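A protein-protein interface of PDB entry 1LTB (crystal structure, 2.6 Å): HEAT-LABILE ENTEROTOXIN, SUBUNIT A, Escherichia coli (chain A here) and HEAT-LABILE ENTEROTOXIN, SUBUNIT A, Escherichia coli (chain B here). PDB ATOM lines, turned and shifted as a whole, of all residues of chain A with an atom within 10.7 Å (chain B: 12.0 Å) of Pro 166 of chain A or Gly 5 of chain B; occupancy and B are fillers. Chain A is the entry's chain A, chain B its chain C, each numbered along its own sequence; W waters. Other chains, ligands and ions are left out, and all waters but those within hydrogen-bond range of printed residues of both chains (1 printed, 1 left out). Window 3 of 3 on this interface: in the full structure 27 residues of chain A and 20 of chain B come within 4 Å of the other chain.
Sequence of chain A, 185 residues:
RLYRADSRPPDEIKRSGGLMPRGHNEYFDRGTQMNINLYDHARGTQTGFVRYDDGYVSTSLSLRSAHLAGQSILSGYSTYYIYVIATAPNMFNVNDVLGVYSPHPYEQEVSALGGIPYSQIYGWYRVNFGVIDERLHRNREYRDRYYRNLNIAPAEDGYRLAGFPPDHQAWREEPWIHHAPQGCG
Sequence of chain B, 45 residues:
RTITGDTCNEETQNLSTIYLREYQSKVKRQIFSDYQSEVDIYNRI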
ATOM      1  N   ASN A  37       6.554  21.032 -28.059  1.00  0.00           N
ATOM      2  CA  ASN A  37       5.446  20.543 -27.225  1.00  0.00           C
ATOM      3  C   ASN A  37       4.792  21.775 -26.639  1.00  0.00           C
ATOM      4  O   ASN A  37       5.368  22.501 -25.812  1.00  0.00           O
ATOM      5  CB  ASN A  37       5.934  19.688 -26.077  1.00  0.00           C
ATOM      6  CG  ASN A  37       4.839  19.213 -25.130  1.00  0.00           C
ATOM      7  OD1 ASN A  37       4.014  19.969 -24.612  1.00  0.00           O
ATOM      8  ND2 ASN A  37       4.775  17.929 -24.834  1.00  0.00           N
ATOM      9  N   TYR A  39       2.290  22.146 -24.547  1.00  0.00           N
ATOM     10  CA  TYR A  39       2.049  22.140 -23.113  1.00  0.00           C
ATOM     11  C   TYR A  39       3.322  22.501 -22.401  1.00  0.00           C
ATOM     12  O   TYR A  39       3.284  23.384 -21.555  1.00  0.00           O
ATOM     13  CB  TYR A  39       1.590  20.768 -22.642  1.00  0.00           C
ATOM     14  CG  TYR A  39       1.172  20.716 -21.176  1.00  0.00           C
ATOM     15  CD1 TYR A  39       0.174  21.555 -20.714  1.00  0.00           C
ATOM     16  CD2 TYR A  39       1.790  19.845 -20.314  1.00  0.00           C
ATOM     17  CE1 TYR A  39      -0.186  21.527 -19.380  1.00  0.00           C
ATOM     18  CE2 TYR A  39       1.427  19.815 -18.980  1.00  0.00           C
ATOM     19  CZ  TYR A  39       0.451  20.659 -18.526  1.00  0.00           C
ATOM     20  OH  TYR A  39       0.082  20.623 -17.205  1.00  0.00           O
ATOM     21  N   ASP A  40       4.440  21.857 -22.706  1.00  0.00           N
ATOM     22  CA  ASP A  40       5.754  22.251 -22.242  1.00  0.00           C
ATOM     23  C   ASP A  40       6.108  23.696 -22.583  1.00  0.00           C
ATOM     24  O   ASP A  40       6.692  24.377 -21.750  1.00  0.00           O
ATOM     25  CB  ASP A  40       6.808  21.358 -22.851  1.00  0.00           C
ATOM     26  CG  ASP A  40       6.935  19.992 -22.187  1.00  0.00           C
ATOM     27  OD1 ASP A  40       6.526  19.830 -21.018  1.00  0.00           O
ATOM     28  OD2 ASP A  40       7.462  19.091 -22.854  1.00  0.00           O
ATOM     29  N   ARG A  43       4.266  26.499 -20.110  1.00  0.00           N
ATOM     30  CA  ARG A  43       4.635  26.455 -18.699  1.00  0.00           C
ATOM     31  C   ARG A  43       6.041  26.933 -18.397  1.00  0.00           C
ATOM     32  O   ARG A  43       6.436  27.099 -17.230  1.00  0.00           O
ATOM     33  CB  ARG A  43       4.571  25.040 -18.129  1.00  0.00           C
ATOM     34  CG  ARG A  43       3.210  24.378 -18.022  1.00  0.00           C
ATOM     35  CD  ARG A  43       3.294  23.038 -17.287  1.00  0.00           C
ATOM     36  NE  ARG A  43       4.242  22.153 -17.959  1.00  0.00           N
ATOM     37  CZ  ARG A  43       4.525  20.900 -17.572  1.00  0.00           C
ATOM     38  NH1 ARG A  43       3.953  20.320 -16.507  1.00  0.00           N
ATOM     39  NH2 ARG A  43       5.419  20.218 -18.306  1.00  0.00           N
ATOM     40  N   ALA A 162      -1.568  19.465 -28.331  1.00  0.00           N
ATOM     41  CA  ALA A 162      -1.437  19.998 -26.988  1.00  0.00           C
ATOM     42  C   ALA A 162      -0.230  19.532 -26.178  1.00  0.00           C
ATOM     43  O   ALA A 162       0.274  20.295 -25.337  1.00  0.00           O
ATOM     44  CB  ALA A 162      -2.670  19.669 -26.198  1.00  0.00           C
ATOM     45  N   GLY A 163       0.273  18.309 -26.375  1.00  0.00           N
ATOM     46  CA  GLY A 163       1.474  17.906 -25.679  1.00  0.00           C
ATOM     47  C   GLY A 163       1.264  17.556 -24.219  1.00  0.00           C
ATOM     48  O   GLY A 163       2.261  17.398 -23.531  1.00  0.00           O
ATOM     49  N   PHE A 164       0.062  17.422 -23.645  1.00  0.00           N
ATOM     50  CA  PHE A 164      -0.107  16.950 -22.242  1.00  0.00           C
ATOM     51  C   PHE A 164       0.548  15.583 -22.026  1.00  0.00           C
ATOM     52  O   PHE A 164       0.550  14.783 -22.973  1.00  0.00           O
ATOM     53  CB  PHE A 164      -1.538  16.703 -21.805  1.00  0.00           C
ATOM     54  CG  PHE A 164      -2.480  17.843 -22.074  1.00  0.00           C
ATOM     55  CD1 PHE A 164      -2.486  18.923 -21.234  1.00  0.00           C
ATOM     56  CD2 PHE A 164      -3.369  17.742 -23.114  1.00  0.00           C
ATOM     57  CE1 PHE A 164      -3.399  19.920 -21.419  1.00  0.00           C
ATOM     58  CE2 PHE A 164      -4.277  18.744 -23.284  1.00  0.00           C
ATOM     59  CZ  PHE A 164      -4.300  19.833 -22.436  1.00  0.00           C
ATOM     60  N   PRO A 165       1.123  15.212 -20.863  1.00  0.00           N
ATOM     61  CA  PRO A 165       1.842  13.945 -20.741  1.00  0.00           C
ATOM     62  C   PRO A 165       0.843  12.814 -20.833  1.00  0.00           C
ATOM     63  O   PRO A 165      -0.352  13.059 -20.593  1.00  0.00           O
ATOM     64  CB  PRO A 165       2.560  14.092 -19.416  1.00  0.00           C
ATOM     65  CG  PRO A 165       1.786  15.126 -18.627  1.00  0.00           C
ATOM     66  CD  PRO A 165       1.395  16.090 -19.718  1.00  0.00           C
ATOM     67  N   PRO A 166       1.258  11.570 -21.148  1.00  0.00           N
ATOM     68  CA  PRO A 166       0.380  10.401 -21.325  1.00  0.00           C
ATOM     69  C   PRO A 166      -0.681  10.161 -20.274  1.00  0.00           C
ATOM     70  O   PRO A 166      -1.755   9.664 -20.583  1.00  0.00           O
ATOM     71  CB  PRO A 166       1.341   9.246 -21.423  1.00  0.00           C
ATOM     72  CG  PRO A 166       2.660   9.761 -20.878  1.00  0.00           C
ATOM     73  CD  PRO A 166       2.655  11.194 -21.358  1.00  0.00           C
ATOM     74  N   ASP A 167      -0.328  10.550 -19.049  1.00  0.00           N
ATOM     75  CA  ASP A 167      -1.133  10.371 -17.881  1.00  0.00           C
ATOM     76  C   ASP A 167      -1.878  11.612 -17.451  1.00  0.00           C
ATOM     77  O   ASP A 167      -2.447  11.688 -16.361  1.00  0.00           O
ATOM     78  CB  ASP A 167      -0.207   9.867 -16.756  1.00  0.00           C
ATOM     79  CG  ASP A 167       0.922  10.771 -16.224  1.00  0.00           C
ATOM     80  OD1 ASP A 167       1.890  11.048 -16.924  1.00  0.00           O
ATOM     81  OD2 ASP A 167       0.841  11.168 -15.071  1.00  0.00           O
ATOM     82  N   HIS A 168      -1.906  12.646 -18.266  1.00  0.00           N
ATOM     83  CA  HIS A 168      -2.525  13.855 -17.789  1.00  0.00           C
ATOM     84  C   HIS A 168      -4.014  13.661 -17.966  1.00  0.00           C
ATOM     85  O   HIS A 168      -4.481  13.280 -19.022  1.00  0.00           O
ATOM     86  CB  HIS A 168      -1.996  15.023 -18.595  1.00  0.00           C
ATOM     87  CG  HIS A 168      -2.523  16.337 -18.089  1.00  0.00           C
ATOM     88  ND1 HIS A 168      -3.776  16.758 -18.140  1.00  0.00           N
ATOM     89  CD2 HIS A 168      -1.804  17.285 -17.421  1.00  0.00           C
ATOM     90  CE1 HIS A 168      -3.854  17.912 -17.512  1.00  0.00           C
ATOM     91  NE2 HIS A 168      -2.664  18.222 -17.085  1.00  0.00           N
ATOM     92  N   GLN A 169      -4.776  13.930 -16.951  1.00  0.00           N
ATOM     93  CA  GLN A 169      -6.223  13.884 -16.994  1.00  0.00           C
ATOM     94  C   GLN A 169      -6.905  14.388 -18.256  1.00  0.00           C
ATOM     95  O   GLN A 169      -7.958  13.895 -18.655  1.00  0.00           O
ATOM     96  CB  GLN A 169      -6.733  14.671 -15.818  1.00  0.00           C
ATOM     97  CG  GLN A 169      -8.199  14.411 -15.527  1.00  0.00           C
ATOM     98  CD  GLN A 169      -8.568  14.805 -14.110  1.00  0.00           C
ATOM     99  OE1 GLN A 169      -9.227  15.821 -13.862  1.00  0.00           O
ATOM    100  NE2 GLN A 169      -8.108  13.988 -13.145  1.00  0.00           N
ATOM    101  N   ALA A 170      -6.348  15.428 -18.865  1.00  0.00           N
ATOM    102  CA  ALA A 170      -6.859  15.951 -20.129  1.00  0.00           C
ATOM    103  C   ALA A 170      -7.138  14.985 -21.270  1.00  0.00           C
ATOM    104  O   ALA A 170      -8.153  15.080 -21.940  1.00  0.00           O
ATOM    105  CB  ALA A 170      -5.903  16.995 -20.647  1.00  0.00           C
ATOM    106  N   TRP A 171      -6.276  14.007 -21.457  1.00  0.00           N
ATOM    107  CA  TRP A 171      -6.425  12.978 -22.473  1.00  0.00           C
ATOM    108  C   TRP A 171      -7.638  12.058 -22.364  1.00  0.00           C
ATOM    109  O   TRP A 171      -7.927  11.229 -23.235  1.00  0.00           O
ATOM    110  CB  TRP A 171      -5.184  12.111 -22.472  1.00  0.00           C
ATOM    111  CG  TRP A 171      -3.991  12.864 -22.998  1.00  0.00           C
ATOM    112  CD1 TRP A 171      -2.798  12.782 -22.340  1.00  0.00           C
ATOM    113  CD2 TRP A 171      -3.951  13.632 -24.150  1.00  0.00           C
ATOM    114  NE1 TRP A 171      -1.990  13.494 -23.084  1.00  0.00           N
ATOM    115  CE2 TRP A 171      -2.619  14.010 -24.162  1.00  0.00           C
ATOM    116  CE3 TRP A 171      -4.799  14.082 -25.168  1.00  0.00           C
ATOM    117  CZ2 TRP A 171      -2.144  14.822 -25.176  1.00  0.00           C
ATOM    118  CZ3 TRP A 171      -4.317  14.885 -26.182  1.00  0.00           C
ATOM    119  CH2 TRP A 171      -2.995  15.252 -26.180  1.00  0.00           C
ATOM    120  N   ARG A 172      -8.328  12.146 -21.233  1.00  0.00           N
ATOM    121  CA  ARG A 172      -9.441  11.265 -20.985  1.00  0.00           C
ATOM    122  C   ARG A 172     -10.707  12.089 -20.918  1.00  0.00           C
ATOM    123  O   ARG A 172     -11.792  11.505 -20.861  1.00  0.00           O
ATOM    124  CB  ARG A 172      -9.208  10.479 -19.680  1.00  0.00           C
ATOM    125  CG  ARG A 172      -7.967   9.571 -19.701  1.00  0.00           C
ATOM    126  CD  ARG A 172      -6.795  10.322 -19.049  1.00  0.00           C
ATOM    127  NE  ARG A 172      -5.461   9.783 -19.320  1.00  0.00           N
ATOM    128  CZ  ARG A 172      -4.697   9.255 -18.352  1.00  0.00           C
ATOM    129  NH1 ARG A 172      -5.096   9.194 -17.066  1.00  0.00           N
ATOM    130  NH2 ARG A 172      -3.526   8.721 -18.697  1.00  0.00           N
ATOM    131  N   GLU A 173     -10.632  13.414 -20.950  1.00  0.00           N
ATOM    132  CA  GLU A 173     -11.857  14.165 -20.988  1.00  0.00           C
ATOM    133  C   GLU A 173     -11.971  14.951 -22.290  1.00  0.00           C
ATOM    134  O   GLU A 173     -11.090  14.947 -23.158  1.00  0.00           O
ATOM    135  CB  GLU A 173     -11.913  15.076 -19.750  1.00  0.00           C
ATOM    136  CG  GLU A 173     -11.013  16.302 -19.782  1.00  0.00           C
ATOM    137  CD  GLU A 173     -10.470  16.724 -18.426  1.00  0.00           C
ATOM    138  OE1 GLU A 173     -10.117  15.841 -17.651  1.00  0.00           O
ATOM    139  OE2 GLU A 173     -10.393  17.927 -18.160  1.00  0.00           O
ATOM    140  N   TRP A 176     -10.087  16.788 -25.743  1.00  0.00           N
ATOM    141  CA  TRP A 176      -8.848  16.110 -26.080  1.00  0.00           C
ATOM    142  C   TRP A 176      -8.975  14.594 -26.275  1.00  0.00           C
ATOM    143  O   TRP A 176      -8.216  14.027 -27.059  1.00  0.00           O
ATOM    144  CB  TRP A 176      -7.822  16.436 -24.980  1.00  0.00           C
ATOM    145  CG  TRP A 176      -7.654  17.912 -24.631  1.00  0.00           C
ATOM    146  CD1 TRP A 176      -6.866  18.649 -25.442  1.00  0.00           C
ATOM    147  CD2 TRP A 176      -8.203  18.648 -23.584  1.00  0.00           C
ATOM    148  NE1 TRP A 176      -6.918  19.848 -24.945  1.00  0.00           N
ATOM    149  CE2 TRP A 176      -7.692  19.905 -23.858  1.00  0.00           C
ATOM    150  CE3 TRP A 176      -9.036  18.543 -22.467  1.00  0.00           C
ATOM    151  CZ2 TRP A 176      -7.971  21.032 -23.079  1.00  0.00           C
ATOM    152  CZ3 TRP A 176      -9.316  19.662 -21.674  1.00  0.00           C
ATOM    153  CH2 TRP A 176      -8.791  20.913 -21.975  1.00  0.00           C
ATOM    154  N   ILE A 177      -9.924  13.891 -25.624  1.00  0.00           N
ATOM    155  CA  ILE A 177     -10.101  12.444 -25.772  1.00  0.00           C
ATOM    156  C   ILE A 177     -10.187  12.090 -27.212  1.00  0.00           C
ATOM    157  O   ILE A 177      -9.550  11.178 -27.734  1.00  0.00           O
ATOM    158  CB  ILE A 177     -11.392  11.799 -25.279  1.00  0.00           C
ATOM    159  CG1 ILE A 177     -12.518  12.801 -25.067  1.00  0.00           C
ATOM    160  CG2 ILE A 177     -10.967  10.941 -24.132  1.00  0.00           C
ATOM    161  CD1 ILE A 177     -13.867  12.220 -24.556  1.00  0.00           C
ATOM    162  N   ALA A 180      -6.584  12.530 -28.848  1.00  0.00           N
ATOM    163  CA  ALA A 180      -5.402  12.040 -28.147  1.00  0.00           C
ATOM    164  C   ALA A 180      -4.506  11.142 -29.004  1.00  0.00           C
ATOM    165  O   ALA A 180      -4.962  10.136 -29.556  1.00  0.00           O
ATOM    166  CB  ALA A 180      -5.834  11.258 -26.901  1.00  0.00           C
ATOM    167  N   PRO A 181      -3.218  11.470 -29.176  1.00  0.00           N
ATOM    168  CA  PRO A 181      -2.281  10.639 -29.902  1.00  0.00           C
ATOM    169  C   PRO A 181      -2.173   9.201 -29.368  1.00  0.00           C
ATOM    170  O   PRO A 181      -2.658   8.793 -28.292  1.00  0.00           O
ATOM    171  CB  PRO A 181      -0.972  11.399 -29.809  1.00  0.00           C
ATOM    172  CG  PRO A 181      -1.361  12.816 -29.523  1.00  0.00           C
ATOM    173  CD  PRO A 181      -2.549  12.646 -28.617  1.00  0.00           C
ATOM    174  N   GLN A 182      -1.456   8.428 -30.180  1.00  0.00           N
ATOM    175  CA  GLN A 182      -1.080   7.086 -29.829  1.00  0.00           C
ATOM    176  C   GLN A 182      -0.155   7.150 -28.617  1.00  0.00           C
ATOM    177  O   GLN A 182       0.988   7.603 -28.657  1.00  0.00           O
ATOM    178  CB  GLN A 182      -0.341   6.406 -30.993  1.00  0.00           C
ATOM    179  CG  GLN A 182      -1.161   6.173 -32.283  1.00  0.00           C
ATOM    180  CD  GLN A 182      -2.199   5.050 -32.206  1.00  0.00           C
ATOM    181  OE1 GLN A 182      -3.356   5.219 -32.576  1.00  0.00           O
ATOM    182  NE2 GLN A 182      -1.857   3.851 -31.734  1.00  0.00           N
ATOM    183  N   GLY A 183      -0.731   6.760 -27.491  1.00  0.00           N
ATOM    184  CA  GLY A 183       0.013   6.573 -26.267  1.00  0.00           C
ATOM    185  C   GLY A 183      -0.313   7.569 -25.170  1.00  0.00           C
ATOM    186  O   GLY A 183       0.468   7.625 -24.190  1.00  0.00           O
ATOM    187  N   CYS A 184      -1.397   8.320 -25.372  1.00  0.00           N
ATOM    188  CA  CYS A 184      -1.867   9.349 -24.477  1.00  0.00           C
ATOM    189  C   CYS A 184      -3.227   8.847 -24.069  1.00  0.00           C
ATOM    190  O   CYS A 184      -4.011   8.573 -24.986  1.00  0.00           O
ATOM    191  CB  CYS A 184      -2.055  10.661 -25.198  1.00  0.00           C
ATOM    192  SG  CYS A 184      -0.601  11.159 -26.115  1.00  0.00           S
ATOM    193  N   GLY A 185      -3.476   8.734 -22.756  1.00  0.00           N
ATOM    194  CA  GLY A 185      -4.735   8.227 -22.207  1.00  0.00           C
ATOM    195  C   GLY A 185      -5.196   6.818 -22.673  1.00  0.00           C
ATOM    196  O   GLY A 185      -4.520   5.788 -22.500  1.00  0.00           O
ATOM    197  N   GLY B   5       2.926   6.686 -23.467  1.00  0.00           N
ATOM    198  CA  GLY B   5       4.203   6.654 -22.752  1.00  0.00           C
ATOM    199  C   GLY B   5       5.142   7.628 -23.460  1.00  0.00           C
ATOM    200  O   GLY B   5       4.590   8.620 -23.940  1.00  0.00           O
ATOM    201  N   ASP B   6       6.455   7.404 -23.643  1.00  0.00           N
ATOM    202  CA  ASP B   6       7.279   8.302 -24.449  1.00  0.00           C
ATOM    203  C   ASP B   6       6.629   8.369 -25.838  1.00  0.00           C
ATOM    204  O   ASP B   6       6.805   9.342 -26.544  1.00  0.00           O
ATOM    205  CB  ASP B   6       8.728   7.777 -24.559  1.00  0.00           C
ATOM    206  CG  ASP B   6       9.037   6.590 -25.495  1.00  0.00           C
ATOM    207  OD1 ASP B   6       8.182   5.723 -25.730  1.00  0.00           O
ATOM    208  OD2 ASP B   6      10.166   6.526 -26.000  1.00  0.00           O
ATOM    209  N   THR B   7       5.849   7.346 -26.236  1.00  0.00           N
ATOM    210  CA  THR B   7       4.982   7.330 -27.424  1.00  0.00           C
ATOM    211  C   THR B   7       4.066   8.545 -27.495  1.00  0.00           C
ATOM    212  O   THR B   7       4.063   9.236 -28.492  1.00  0.00           O
ATOM    213  CB  THR B   7       4.115   6.060 -27.419  1.00  0.00           C
ATOM    214  OG1 THR B   7       5.049   5.080 -26.985  1.00  0.00           O
ATOM    215  CG2 THR B   7       3.433   5.677 -28.731  1.00  0.00           C
ATOM    216  N   CYS B   8       3.384   8.905 -26.420  1.00  0.00           N
ATOM    217  CA  CYS B   8       2.519  10.062 -26.364  1.00  0.00           C
ATOM    218  C   CYS B   8       3.358  11.254 -26.740  1.00  0.00           C
ATOM    219  O   CYS B   8       2.935  12.016 -27.604  1.00  0.00           O
ATOM    220  CB  CYS B   8       2.040  10.207 -24.982  1.00  0.00           C
ATOM    221  SG  CYS B   8       0.825  11.492 -24.730  1.00  0.00           S
ATOM    222  N   ASN B   9       4.590  11.325 -26.211  1.00  0.00           N
ATOM    223  CA  ASN B   9       5.515  12.416 -26.498  1.00  0.00           C
ATOM    224  C   ASN B   9       6.231  12.284 -27.826  1.00  0.00           C
ATOM    225  O   ASN B   9       6.634  13.320 -28.359  1.00  0.00           O
ATOM    226  CB  ASN B   9       6.615  12.570 -25.451  1.00  0.00           C
ATOM    227  CG  ASN B   9       6.036  12.669 -24.057  1.00  0.00           C
ATOM    228  OD1 ASN B   9       6.218  11.746 -23.263  1.00  0.00           O
ATOM    229  ND2 ASN B   9       5.210  13.642 -23.681  1.00  0.00           N
ATOM    230  N   GLU B  10       6.403  11.108 -28.435  1.00  0.00           N
ATOM    231  CA  GLU B  10       7.072  10.996 -29.716  1.00  0.00           C
ATOM    232  C   GLU B  10       6.016  11.318 -30.724  1.00  0.00           C
ATOM    233  O   GLU B  10       6.231  12.182 -31.564  1.00  0.00           O
ATOM    234  CB  GLU B  10       7.594   9.611 -29.969  1.00  0.00           C
ATOM    235  CG  GLU B  10       8.802   9.414 -29.069  1.00  0.00           C
ATOM    236  CD  GLU B  10       9.455   8.031 -29.144  1.00  0.00           C
ATOM    237  OE1 GLU B  10       8.764   7.028 -28.894  1.00  0.00           O
ATOM    238  OE2 GLU B  10      10.664   7.969 -29.437  1.00  0.00           O
ATOM    239  N   GLU B  11       4.849  10.693 -30.642  1.00  0.00           N
ATOM    240  CA  GLU B  11       3.712  11.003 -31.462  1.00  0.00           C
ATOM    241  C   GLU B  11       3.415  12.494 -31.421  1.00  0.00           C
ATOM    242  O   GLU B  11       3.145  13.045 -32.482  1.00  0.00           O
ATOM    243  CB  GLU B  11       2.515  10.250 -30.981  1.00  0.00           C
ATOM    244  CG  GLU B  11       1.465  10.055 -32.073  1.00  0.00           C
ATOM    245  CD  GLU B  11       1.717   8.979 -33.125  1.00  0.00           C
ATOM    246  OE1 GLU B  11       2.763   8.329 -33.127  1.00  0.00           O
ATOM    247  OE2 GLU B  11       0.837   8.775 -33.953  1.00  0.00           O
ATOM    248  N   THR B  12       3.490  13.205 -30.294  1.00  0.00           N
ATOM    249  CA  THR B  12       3.329  14.663 -30.267  1.00  0.00           C
ATOM    250  C   THR B  12       4.416  15.384 -31.094  1.00  0.00           C
ATOM    251  O   THR B  12       4.142  16.263 -31.920  1.00  0.00           O
ATOM    252  CB  THR B  12       3.381  15.208 -28.807  1.00  0.00           C
ATOM    253  OG1 THR B  12       2.263  14.664 -28.097  1.00  0.00           O
ATOM    254  CG2 THR B  12       3.359  16.753 -28.774  1.00  0.00           C
ATOM    255  N   GLN B  13       5.676  15.004 -30.945  1.00  0.00           N
ATOM    256  CA  GLN B  13       6.745  15.618 -31.692  1.00  0.00           C
ATOM    257  C   GLN B  13       6.693  15.413 -33.196  1.00  0.00           C
ATOM    258  O   GLN B  13       6.949  16.301 -34.000  1.00  0.00           O
ATOM    259  CB  GLN B  13       8.005  15.085 -31.113  1.00  0.00           C
ATOM    260  CG  GLN B  13       8.467  16.285 -30.386  1.00  0.00           C
ATOM    261  CD  GLN B  13       9.598  16.964 -31.115  1.00  0.00           C
ATOM    262  OE1 GLN B  13      10.552  17.213 -30.413  1.00  0.00           O
ATOM    263  NE2 GLN B  13       9.723  17.321 -32.387  1.00  0.00           N
ATOM    264  N   ASN B  14       6.311  14.203 -33.551  1.00  0.00           N
ATOM    265  CA  ASN B  14       6.160  13.707 -34.896  1.00  0.00           C
ATOM    266  C   ASN B  14       4.928  14.360 -35.517  1.00  0.00           C
ATOM    267  O   ASN B  14       5.020  14.793 -36.662  1.00  0.00           O
ATOM    268  CB  ASN B  14       6.108  12.189 -34.680  1.00  0.00           C
ATOM    269  CG  ASN B  14       5.577  11.300 -35.787  1.00  0.00           C
ATOM    270  OD1 ASN B  14       6.263  11.055 -36.776  1.00  0.00           O
ATOM    271  ND2 ASN B  14       4.389  10.705 -35.689  1.00  0.00           N
ATOM    272  N   LEU B  15       3.775  14.557 -34.867  1.00  0.00           N
ATOM    273  CA  LEU B  15       2.631  15.207 -35.505  1.00  0.00           C
ATOM    274  C   LEU B  15       2.880  16.693 -35.623  1.00  0.00           C
ATOM    275  O   LEU B  15       2.445  17.307 -36.604  1.00  0.00           O
ATOM    276  CB  LEU B  15       1.368  15.042 -34.714  1.00  0.00           C
ATOM    277  CG  LEU B  15       0.944  13.620 -34.361  1.00  0.00           C
ATOM    278  CD1 LEU B  15      -0.096  13.698 -33.253  1.00  0.00           C
ATOM    279  CD2 LEU B  15       0.481  12.877 -35.603  1.00  0.00           C
HETATM  280  O   HOH W   1      -0.209  15.999 -27.929  1.00  0.00           O
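Among the printed residues, merely in contact across the chains: Gly 183 of chain A with Cys 8 of chain B, Gln 182 of chain A with Cys 8 of chain B, Pro 181 of chain A with Glu 11 of chain B, Pro 166 of chain A with Gly 5 of chain B, Gln 182 of chain A with Glu 11 of chain B, Gly 163 of chain A with Thr 12 of chain B and Trp 171 of chain A with Cys 8 of chain B.
The backbone carbonyl oxygen (O) of Phe 164 of chain A sits at hydrogen-bond distance from the indole nitrogen (NE1) of Trp 171 of chain A (2.9 Å). OG1 of Thr 12 of chain B sits at hydrogen-bond distance from O of Cys 8 of chain B (2.8 Å). The backbone NH (N) of Gly 185 of chain A is in hydrogen-bond range of the backbone carbonyl oxygen (O) of Pro 166 of chain A (2.9 Å). O of Pro 166 of chain A sits at hydrogen-bond distance from NH2 of Arg 172 of chain A. O of Pro 165 of chain A lies within hydrogen-bond range of NE1 of Trp 171 of chain A, at 3.0 Å. O of Gly 163 of chain A is in hydrogen-bond range of ND2 of Asn 37 of chain A (2.9 Å).
Of the 24 printed residues of chain A, 8 touch a printed residue of chain B. Of the 11 printed residues of chain B, 5 touch a printed residue of chain A. Printed residues of chain B that touch a printed residue of chain A: Gly 5, Thr 7, Cys 8, Glu 11 and Thr 12.
Of chain A, only Pro 166 and Gly 183 come within 4 Å of Gly 5 of chain B. No residue of chain B comes within 4 Å of Pro 165 of chain A. No residue of chain B comes within 4 Å of Asp 167 of chain A. No residue of chain B comes within 4 Å of Gly 185 of chain A. Asp 6 of chain B touches none of the printed residues of chain A. Thr 7 of chain B touches just one residue of chain A: Gln 182 (3.1 Å). Of the printed residues of chain A, Cys 8 of chain B touches Phe 164, Pro 166, Trp 171, Gln 182, Gly 183 and Cys 184. Of the printed residues of chain B, Trp 171 of chain A touches Cys 8. Of the printed residues of chain B, Pro 181 of chain A touches Glu 11. Printed residues of chain B within 4 Å of Gln 182 of chain A: Thr 7, Cys 8 and Glu 11. Printed residues of chain A within 4 Å of Thr 12 of chain B: Gly 163. Ala 162 of chain A touches none of the printed residues of chain B. The nearest residue of chain A that does not touch Gly 5 of chain B is Cys 184 of chain A (5.0 Å). The nearest printed residue of chain A that does not touch Glu 11 of chain B is Cys 184 of chain A (5.8 Å).
Water W1 bridges the side-chain hydroxyl of Thr 12 of chain B and the backbone NH of Gly 163 of chain A.
O of Gln 182 of chain A sits close to O of Thr 7 of chain B, at 3.5 Å. The backbone carbonyl oxygen (O) of Gly 183 of chain A sits at hydrogen-bond distance from the backbone NH (N) of Gly 5 of chain B (2.7 Å). N of Pro 166 of chain A lies close to SG of Cys 8 of chain B. The side-chain sulfur (SG) of Cys 8 of chain B is disulfide-bonded to the side-chain sulfur (SG) of Cys 184 of chain A, 2.0 Å away. O of Phe 164 of chain A sits close to SG of Cys 8 of chain B.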
